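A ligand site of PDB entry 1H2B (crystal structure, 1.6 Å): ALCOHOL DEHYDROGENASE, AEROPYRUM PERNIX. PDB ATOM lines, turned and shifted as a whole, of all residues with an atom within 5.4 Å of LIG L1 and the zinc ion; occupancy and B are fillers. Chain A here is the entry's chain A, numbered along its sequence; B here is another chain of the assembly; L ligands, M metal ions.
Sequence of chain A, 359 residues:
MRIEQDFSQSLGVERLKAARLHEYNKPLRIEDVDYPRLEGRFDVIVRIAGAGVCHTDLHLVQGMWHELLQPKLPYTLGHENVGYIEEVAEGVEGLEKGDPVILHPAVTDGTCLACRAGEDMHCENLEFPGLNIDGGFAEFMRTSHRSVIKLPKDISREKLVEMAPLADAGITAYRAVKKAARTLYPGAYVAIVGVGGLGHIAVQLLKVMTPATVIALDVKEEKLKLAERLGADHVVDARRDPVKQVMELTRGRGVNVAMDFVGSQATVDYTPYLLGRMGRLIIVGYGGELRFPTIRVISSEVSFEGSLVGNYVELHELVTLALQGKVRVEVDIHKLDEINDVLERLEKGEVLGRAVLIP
OG1 of Thr 56 lies close to O1 of LIG L1, 2.7 Å away. O13 of LG2 L2 sits at hydrogen-bond distance from N of Thr 56 (3.5 Å). The side-chain hydroxyl (OG1) of Thr 56 is in hydrogen-bond range of an oxygen (O13) of LG2 L2 (3.0 Å). The backbone NH (N) of Val 309 sits at hydrogen-bond distance from an oxygen (O14) of LG2 L2, at 2.7 Å. The guanidinium group (NH1) of Arg 354 lies within salt-bridge range of an oxygen (O8) of LG2 L2, 2.6 Å away. O12 of LG2 L2 sits at hydrogen-bond distance from N of Tyr 286 (3.2 Å). O of Tyr 286 is in hydrogen-bond range of O12 of LG2 L2 (3.5 Å).
The backbone carbonyl oxygen (O) of Asp 168 is in hydrogen-bond range of the side-chain hydroxyl (OG1) of Thr 172 (2.7 Å). SG of Cys 54 sits close to N of Thr 56 (3.4 Å). The side-chain sulfur (SG) of Cys 54 sits close to the guanidinium group (NH2) of Arg 354, at 3.3 Å. OG1 of Thr 56 is in hydrogen-bond range of OH of Tyr 286 (2.8 Å). The backbone carbonyl oxygen of Ser 299 of chain B is in hydrogen-bond range of the guanidinium group of Arg 277 of chain B (2.8 Å). The guanidinium group (NH2) of Arg 277 of chain B lies within hydrogen-bond range of the backbone carbonyl oxygen (O) of Met 121, 3.1 Å away. The side-chain hydroxyl (OH) of Tyr 286 is in hydrogen-bond range of the indole nitrogen (NE1) of Trp 65 (2.9 Å).
Residues that only touch LIG L1: Ser 299 of chain B, Arg 277 of chain B, Phe 128, Leu 131, Val 309, Leu 308 and Trp 65. The nearest printed residue that does not touch LIG L1 is Met 121 (4.2 Å).
Residues that only touch the zinc ion: Thr 56. Four residues have an atom within 4 Å of the zinc ion: Cys 54, Thr 56, His 79 and Asp 168.
The zinc ion is bound by O1 of LIG L1 (1.9 Å), NE2 of His 79 (2.0 Å), OD1 of Asp 168 (2.1 Å) and SG of Cys 54 (2.3 Å).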
ATOM      1  N   CYS A  54      25.505  -0.481 -20.138  1.00  0.00           N
ATOM      2  CA  CYS A  54      26.460  -1.536 -20.406  1.00  0.00           C
ATOM      3  C   CYS A  54      27.797  -0.956 -20.884  1.00  0.00           C
ATOM      4  O   CYS A  54      27.821   0.117 -21.473  1.00  0.00           O
ATOM      5  CB  CYS A  54      25.875  -2.434 -21.512  1.00  0.00           C
ATOM      6  SG  CYS A  54      26.850  -3.876 -21.975  1.00  0.00           S
ATOM      7  N   THR A  56      29.174  -1.863 -23.399  1.00  0.00           N
ATOM      8  CA  THR A  56      28.950  -1.760 -24.851  1.00  0.00           C
ATOM      9  C   THR A  56      28.516  -0.359 -25.231  1.00  0.00           C
ATOM     10  O   THR A  56      28.822   0.094 -26.354  1.00  0.00           O
ATOM     11  CB  THR A  56      27.917  -2.810 -25.280  1.00  0.00           C
ATOM     12  OG1 THR A  56      28.571  -4.083 -25.304  1.00  0.00           O
ATOM     13  CG2 THR A  56      27.390  -2.569 -26.718  1.00  0.00           C
ATOM     14  N   TRP A  65      31.297   0.126 -33.204  1.00  0.00           N
ATOM     15  CA  TRP A  65      30.319  -0.660 -33.944  1.00  0.00           C
ATOM     16  C   TRP A  65      29.906  -0.019 -35.282  1.00  0.00           C
ATOM     17  O   TRP A  65      29.067  -0.575 -35.996  1.00  0.00           O
ATOM     18  CB  TRP A  65      29.067  -0.879 -33.100  1.00  0.00           C
ATOM     19  CG  TRP A  65      29.302  -1.904 -32.028  1.00  0.00           C
ATOM     20  CD1 TRP A  65      29.579  -1.662 -30.688  1.00  0.00           C
ATOM     21  CD2 TRP A  65      29.288  -3.310 -32.181  1.00  0.00           C
ATOM     22  NE1 TRP A  65      29.718  -2.853 -30.011  1.00  0.00           N
ATOM     23  CE2 TRP A  65      29.561  -3.887 -30.902  1.00  0.00           C
ATOM     24  CE3 TRP A  65      29.064  -4.181 -33.268  1.00  0.00           C
ATOM     25  CZ2 TRP A  65      29.602  -5.265 -30.688  1.00  0.00           C
ATOM     26  CZ3 TRP A  65      29.114  -5.561 -33.036  1.00  0.00           C
ATOM     27  CH2 TRP A  65      29.390  -6.074 -31.763  1.00  0.00           C
ATOM     28  N   HIS A  79      20.014  -1.183 -24.121  1.00  0.00           N
ATOM     29  CA  HIS A  79      19.583  -2.529 -24.602  1.00  0.00           C
ATOM     30  C   HIS A  79      19.344  -3.532 -23.457  1.00  0.00           C
ATOM     31  O   HIS A  79      19.295  -4.767 -23.687  1.00  0.00           O
ATOM     32  CB  HIS A  79      20.610  -3.087 -25.609  1.00  0.00           C
ATOM     33  CG  HIS A  79      22.021  -3.138 -25.098  1.00  0.00           C
ATOM     34  ND1 HIS A  79      22.876  -2.059 -25.160  1.00  0.00           N
ATOM     35  CD2 HIS A  79      22.721  -4.144 -24.515  1.00  0.00           C
ATOM     36  CE1 HIS A  79      24.040  -2.392 -24.627  1.00  0.00           C
ATOM     37  NE2 HIS A  79      23.990  -3.659 -24.236  1.00  0.00           N
ATOM     38  N   GLU A  80      19.186  -2.986 -22.255  1.00  0.00           N
ATOM     39  CA  GLU A  80      19.045  -3.806 -21.038  1.00  0.00           C
ATOM     40  C   GLU A  80      17.828  -3.381 -20.243  1.00  0.00           C
ATOM     41  O   GLU A  80      17.909  -2.642 -19.236  1.00  0.00           O
ATOM     42  CB  GLU A  80      20.315  -3.624 -20.201  1.00  0.00           C
ATOM     43  CG  GLU A  80      20.490  -4.666 -19.092  1.00  0.00           C
ATOM     44  CD  GLU A  80      21.920  -4.633 -18.570  1.00  0.00           C
ATOM     45  OE1 GLU A  80      22.176  -3.832 -17.650  1.00  0.00           O
ATOM     46  OE2 GLU A  80      22.786  -5.403 -19.054  1.00  0.00           O
ATOM     47  N   MET A 121      20.224 -15.087 -31.387  1.00  0.00           N
ATOM     48  CA  MET A 121      21.249 -14.119 -31.787  1.00  0.00           C
ATOM     49  C   MET A 121      21.798 -14.415 -33.139  1.00  0.00           C
ATOM     50  O   MET A 121      22.622 -13.652 -33.665  1.00  0.00           O
ATOM     51  CB  MET A 121      22.411 -14.096 -30.759  1.00  0.00           C
ATOM     52  CG  MET A 121      21.962 -13.693 -29.355  1.00  0.00           C
ATOM     53  SD  MET A 121      21.213 -12.070 -29.327  1.00  0.00           S
ATOM     54  CE  MET A 121      22.537 -11.016 -30.083  1.00  0.00           C
ATOM     55  N   LEU A 126      17.998 -10.008 -37.705  1.00  0.00           N
ATOM     56  CA  LEU A 126      18.105  -9.467 -36.341  1.00  0.00           C
ATOM     57  C   LEU A 126      18.106  -7.930 -36.291  1.00  0.00           C
ATOM     58  O   LEU A 126      18.878  -7.268 -37.014  1.00  0.00           O
ATOM     59  CB  LEU A 126      19.373 -10.029 -35.670  1.00  0.00           C
ATOM     60  CG  LEU A 126      19.351  -9.793 -34.154  1.00  0.00           C
ATOM     61  CD1 LEU A 126      19.665 -11.070 -33.425  1.00  0.00           C
ATOM     62  CD2 LEU A 126      20.310  -8.675 -33.760  1.00  0.00           C
ATOM     63  N   PHE A 128      18.305  -4.898 -32.960  1.00  0.00           N
ATOM     64  CA  PHE A 128      18.756  -4.897 -31.583  1.00  0.00           C
ATOM     65  C   PHE A 128      18.542  -3.502 -30.988  1.00  0.00           C
ATOM     66  O   PHE A 128      19.412  -2.634 -31.146  1.00  0.00           O
ATOM     67  CB  PHE A 128      20.231  -5.308 -31.620  1.00  0.00           C
ATOM     68  CG  PHE A 128      20.765  -5.891 -30.321  1.00  0.00           C
ATOM     69  CD1 PHE A 128      21.015  -7.250 -30.195  1.00  0.00           C
ATOM     70  CD2 PHE A 128      21.056  -5.079 -29.228  1.00  0.00           C
ATOM     71  CE1 PHE A 128      21.535  -7.810 -28.988  1.00  0.00           C
ATOM     72  CE2 PHE A 128      21.591  -5.615 -28.038  1.00  0.00           C
ATOM     73  CZ  PHE A 128      21.838  -6.974 -27.920  1.00  0.00           C
ATOM     74  N   LEU A 131      21.319  -0.817 -29.986  1.00  0.00           N
ATOM     75  CA  LEU A 131      22.584  -1.074 -30.685  1.00  0.00           C
ATOM     76  C   LEU A 131      22.581  -0.498 -32.071  1.00  0.00           C
ATOM     77  O   LEU A 131      23.480   0.264 -32.388  1.00  0.00           O
ATOM     78  CB  LEU A 131      22.961  -2.567 -30.745  1.00  0.00           C
ATOM     79  CG  LEU A 131      24.188  -2.691 -29.819  1.00  0.00           C
ATOM     80  CD1 LEU A 131      23.821  -3.073 -28.392  1.00  0.00           C
ATOM     81  CD2 LEU A 131      25.309  -3.530 -30.366  1.00  0.00           C
ATOM     82  N   ASP A 168      20.712  -8.342 -20.342  1.00  0.00           N
ATOM     83  CA  ASP A 168      21.878  -8.341 -21.201  1.00  0.00           C
ATOM     84  C   ASP A 168      23.110  -8.798 -20.435  1.00  0.00           C
ATOM     85  O   ASP A 168      23.721  -9.804 -20.778  1.00  0.00           O
ATOM     86  CB  ASP A 168      22.054  -6.932 -21.827  1.00  0.00           C
ATOM     87  CG  ASP A 168      23.186  -6.892 -22.788  1.00  0.00           C
ATOM     88  OD1 ASP A 168      24.192  -6.243 -22.477  1.00  0.00           O
ATOM     89  OD2 ASP A 168      23.190  -7.534 -23.860  1.00  0.00           O
ATOM     90  N   THR A 172      24.054 -12.772 -20.860  1.00  0.00           N
ATOM     91  CA  THR A 172      25.371 -13.009 -21.482  1.00  0.00           C
ATOM     92  C   THR A 172      26.270 -13.818 -20.550  1.00  0.00           C
ATOM     93  O   THR A 172      26.890 -14.803 -20.973  1.00  0.00           O
ATOM     94  CB  THR A 172      26.051 -11.695 -21.814  1.00  0.00           C
ATOM     95  OG1 THR A 172      25.219 -10.976 -22.710  1.00  0.00           O
ATOM     96  CG2 THR A 172      27.363 -11.936 -22.546  1.00  0.00           C
ATOM     97  N   TYR A 286      34.954  -7.510 -25.390  1.00  0.00           N
ATOM     98  CA  TYR A 286      35.641  -7.325 -26.669  1.00  0.00           C
ATOM     99  C   TYR A 286      36.219  -5.928 -26.731  1.00  0.00           C
ATOM    100  O   TYR A 286      35.945  -5.072 -25.920  1.00  0.00           O
ATOM    101  CB  TYR A 286      34.665  -7.586 -27.832  1.00  0.00           C
ATOM    102  CG  TYR A 286      33.486  -6.649 -27.782  1.00  0.00           C
ATOM    103  CD1 TYR A 286      33.510  -5.408 -28.409  1.00  0.00           C
ATOM    104  CD2 TYR A 286      32.333  -6.998 -27.066  1.00  0.00           C
ATOM    105  CE1 TYR A 286      32.422  -4.540 -28.320  1.00  0.00           C
ATOM    106  CE2 TYR A 286      31.236  -6.131 -26.962  1.00  0.00           C
ATOM    107  CZ  TYR A 286      31.307  -4.892 -27.590  1.00  0.00           C
ATOM    108  OH  TYR A 286      30.289  -4.020 -27.467  1.00  0.00           O
ATOM    109  N   LEU A 308      27.972 -14.937 -27.206  1.00  0.00           N
ATOM    110  CA  LEU A 308      27.222 -13.781 -27.639  1.00  0.00           C
ATOM    111  C   LEU A 308      25.846 -13.730 -26.987  1.00  0.00           C
ATOM    112  O   LEU A 308      24.964 -14.560 -27.297  1.00  0.00           O
ATOM    113  CB  LEU A 308      27.102 -13.814 -29.178  1.00  0.00           C
ATOM    114  CG  LEU A 308      26.207 -12.729 -29.805  1.00  0.00           C
ATOM    115  CD1 LEU A 308      26.816 -11.331 -29.604  1.00  0.00           C
ATOM    116  CD2 LEU A 308      25.973 -13.006 -31.303  1.00  0.00           C
ATOM    117  N   VAL A 309      25.662 -12.749 -26.093  1.00  0.00           N
ATOM    118  CA  VAL A 309      24.372 -12.537 -25.431  1.00  0.00           C
ATOM    119  C   VAL A 309      23.792 -13.894 -25.041  1.00  0.00           C
ATOM    120  O   VAL A 309      24.464 -14.662 -24.352  1.00  0.00           O
ATOM    121  CB  VAL A 309      23.426 -11.570 -26.224  1.00  0.00           C
ATOM    122  CG1 VAL A 309      22.296 -11.028 -25.337  1.00  0.00           C
ATOM    123  CG2 VAL A 309      24.231 -10.348 -26.792  1.00  0.00           C
ATOM    124  N   ARG A 354      26.352  -2.976 -11.597  1.00  0.00           N
ATOM    125  CA  ARG A 354      25.644  -2.459 -12.774  1.00  0.00           C
ATOM    126  C   ARG A 354      24.855  -1.211 -12.476  1.00  0.00           C
ATOM    127  O   ARG A 354      24.032  -1.212 -11.603  1.00  0.00           O
ATOM    128  CB  ARG A 354      24.665  -3.530 -13.286  1.00  0.00           C
ATOM    129  CG  ARG A 354      24.108  -3.334 -14.692  1.00  0.00           C
ATOM    130  CD  ARG A 354      25.145  -3.071 -15.740  1.00  0.00           C
ATOM    131  NE  ARG A 354      24.864  -3.711 -16.998  1.00  0.00           N
ATOM    132  CZ  ARG A 354      25.830  -3.990 -17.868  1.00  0.00           C
ATOM    133  NH1 ARG A 354      27.108  -3.719 -17.583  1.00  0.00           N
ATOM    134  NH2 ARG A 354      25.475  -4.560 -19.028  1.00  0.00           N
ATOM    135  N   ARG B 277      28.520 -17.863 -38.958  1.00  0.00           N
ATOM    136  CA  ARG B 277      28.029 -17.641 -37.586  1.00  0.00           C
ATOM    137  C   ARG B 277      28.090 -18.950 -36.851  1.00  0.00           C
ATOM    138  O   ARG B 277      27.684 -20.038 -37.361  1.00  0.00           O
ATOM    139  CB  ARG B 277      26.607 -17.099 -37.594  1.00  0.00           C
ATOM    140  CG  ARG B 277      26.518 -15.715 -38.219  1.00  0.00           C
ATOM    141  CD  ARG B 277      25.164 -14.996 -38.007  1.00  0.00           C
ATOM    142  NE  ARG B 277      25.036 -14.480 -36.645  1.00  0.00           N
ATOM    143  CZ  ARG B 277      25.678 -13.416 -36.150  1.00  0.00           C
ATOM    144  NH1 ARG B 277      26.496 -12.661 -36.885  1.00  0.00           N
ATOM    145  NH2 ARG B 277      25.467 -13.075 -34.876  1.00  0.00           N
ATOM    146  N   ILE B 298      33.110 -12.335 -30.829  1.00  0.00           N
ATOM    147  CA  ILE B 298      31.791 -12.349 -30.177  1.00  0.00           C
ATOM    148  C   ILE B 298      30.658 -12.084 -31.177  1.00  0.00           C
ATOM    149  O   ILE B 298      29.599 -12.731 -31.072  1.00  0.00           O
ATOM    150  CB  ILE B 298      31.755 -11.444 -28.895  1.00  0.00           C
ATOM    151  CG1 ILE B 298      31.733  -9.960 -29.240  1.00  0.00           C
ATOM    152  CG2 ILE B 298      32.923 -11.780 -27.975  1.00  0.00           C
ATOM    153  CD1 ILE B 298      30.350  -9.347 -29.393  1.00  0.00           C
ATOM    154  N   SER B 299      30.829 -11.183 -32.143  1.00  0.00           N
ATOM    155  CA  SER B 299      29.659 -10.847 -32.985  1.00  0.00           C
ATOM    156  C   SER B 299      29.254 -12.010 -33.893  1.00  0.00           C
ATOM    157  O   SER B 299      28.067 -12.124 -34.206  1.00  0.00           O
ATOM    158  CB  SER B 299      29.833  -9.539 -33.754  1.00  0.00           C
ATOM    159  OG  SER B 299      30.933  -9.680 -34.596  1.00  0.00           O
HETATM  160  C1  LIG L   1      25.797  -6.301 -25.925  1.00  0.00           C
HETATM  161  C2  LIG L   1      26.586  -6.566 -27.199  1.00  0.00           C
HETATM  162  C3  LIG L   1      25.689  -7.224 -28.253  1.00  0.00           C
HETATM  163  C4  LIG L   1      26.213  -7.050 -29.677  1.00  0.00           C
HETATM  164  C5  LIG L   1      25.311  -7.846 -30.621  1.00  0.00           C
HETATM  165  C6  LIG L   1      26.052  -8.260 -31.888  1.00  0.00           C
HETATM  166  C7  LIG L   1      25.046  -8.834 -32.904  1.00  0.00           C
HETATM  167  C8  LIG L   1      25.669  -9.845 -33.865  1.00  0.00           C
HETATM  168  O1  LIG L   1      26.290  -5.506 -25.052  1.00  0.00           O
HETATM  169  O2  LIG L   1      24.651  -6.807 -25.797  1.00  0.00           O
HETATM  170  P1  LG2 L   2      32.259  -3.232 -16.867  1.00  0.00           P
HETATM  171  O1  LG2 L   2      32.938  -1.914 -17.232  1.00  0.00           O
HETATM  172  O2  LG2 L   2      31.107  -3.175 -15.876  1.00  0.00           O
HETATM  173  O3  LG2 L   2      33.270  -4.249 -16.222  1.00  0.00           O
HETATM  174  C1  LG2 L   2      34.612  -4.426 -16.672  1.00  0.00           C
HETATM  175  C2  LG2 L   2      35.367  -4.975 -15.465  1.00  0.00           C
HETATM  176  O4  LG2 L   2      36.682  -5.268 -15.881  1.00  0.00           O
HETATM  177  C3  LG2 L   2      35.526  -3.939 -14.308  1.00  0.00           C
HETATM  178  O5  LG2 L   2      35.093  -4.493 -13.078  1.00  0.00           O
HETATM  179  C4  LG2 L   2      36.986  -3.555 -14.409  1.00  0.00           C
HETATM  180  O6  LG2 L   2      37.574  -3.033 -13.221  1.00  0.00           O
HETATM  181  C5  LG2 L   2      37.600  -4.863 -14.863  1.00  0.00           C
HETATM  182  N1  LG2 L   2      38.915  -4.691 -15.463  1.00  0.00           N
HETATM  183  C6  LG2 L   2      39.429  -3.653 -16.212  1.00  0.00           C
HETATM  184  N2  LG2 L   2      40.682  -3.985 -16.580  1.00  0.00           N
HETATM  185  C7  LG2 L   2      40.983  -5.226 -16.075  1.00  0.00           C
HETATM  186  C8  LG2 L   2      42.115  -6.030 -16.100  1.00  0.00           C
HETATM  187  N3  LG2 L   2      43.247  -5.674 -16.727  1.00  0.00           N
HETATM  188  N4  LG2 L   2      42.093  -7.276 -15.486  1.00  0.00           N
HETATM  189  C9  LG2 L   2      40.941  -7.646 -14.784  1.00  0.00           C
HETATM  190  N5  LG2 L   2      39.845  -6.866 -14.734  1.00  0.00           N
HETATM  191  C10 LG2 L   2      39.858  -5.660 -15.371  1.00  0.00           C
HETATM  192  O7  LG2 L   2      31.821  -3.862 -18.272  1.00  0.00           O
HETATM  193  P2  LG2 L   2      30.561  -4.812 -18.594  1.00  0.00           P
HETATM  194  O8  LG2 L   2      29.398  -3.962 -18.894  1.00  0.00           O
HETATM  195  O9  LG2 L   2      30.535  -5.884 -17.580  1.00  0.00           O
HETATM  196  O10 LG2 L   2      31.071  -5.417 -19.982  1.00  0.00           O
HETATM  197  C11 LG2 L   2      32.192  -6.287 -19.986  1.00  0.00           C
HETATM  198  C12 LG2 L   2      32.685  -6.560 -21.420  1.00  0.00           C
HETATM  199  O11 LG2 L   2      31.686  -7.383 -22.075  1.00  0.00           O
HETATM  200  C13 LG2 L   2      32.730  -5.296 -22.300  1.00  0.00           C
HETATM  201  O12 LG2 L   2      33.770  -5.455 -23.237  1.00  0.00           O
HETATM  202  C14 LG2 L   2      31.375  -5.251 -22.972  1.00  0.00           C
HETATM  203  O13 LG2 L   2      31.330  -4.469 -24.137  1.00  0.00           O
HETATM  204  C15 LG2 L   2      31.236  -6.741 -23.262  1.00  0.00           C
HETATM  205  N6  LG2 L   2      29.889  -7.233 -23.605  1.00  0.00           N
HETATM  206  C16 LG2 L   2      29.867  -8.399 -24.318  1.00  0.00           C
HETATM  207  C17 LG2 L   2      28.652  -9.000 -24.591  1.00  0.00           C
HETATM  208  C18 LG2 L   2      28.651 -10.245 -25.445  1.00  0.00           C
HETATM  209  O14 LG2 L   2      27.452 -10.707 -25.755  1.00  0.00           O
HETATM  210  N7  LG2 L   2      29.764 -10.827 -25.861  1.00  0.00           N
HETATM  211  C19 LG2 L   2      27.417  -8.489 -24.091  1.00  0.00           C
HETATM  212  C20 LG2 L   2      27.497  -7.375 -23.210  1.00  0.00           C
HETATM  213  C21 LG2 L   2      28.735  -6.793 -22.973  1.00  0.00           C
HETATM  214 ZN    ZN M   1      25.435  -4.825 -23.446  1.00  0.00          ZN
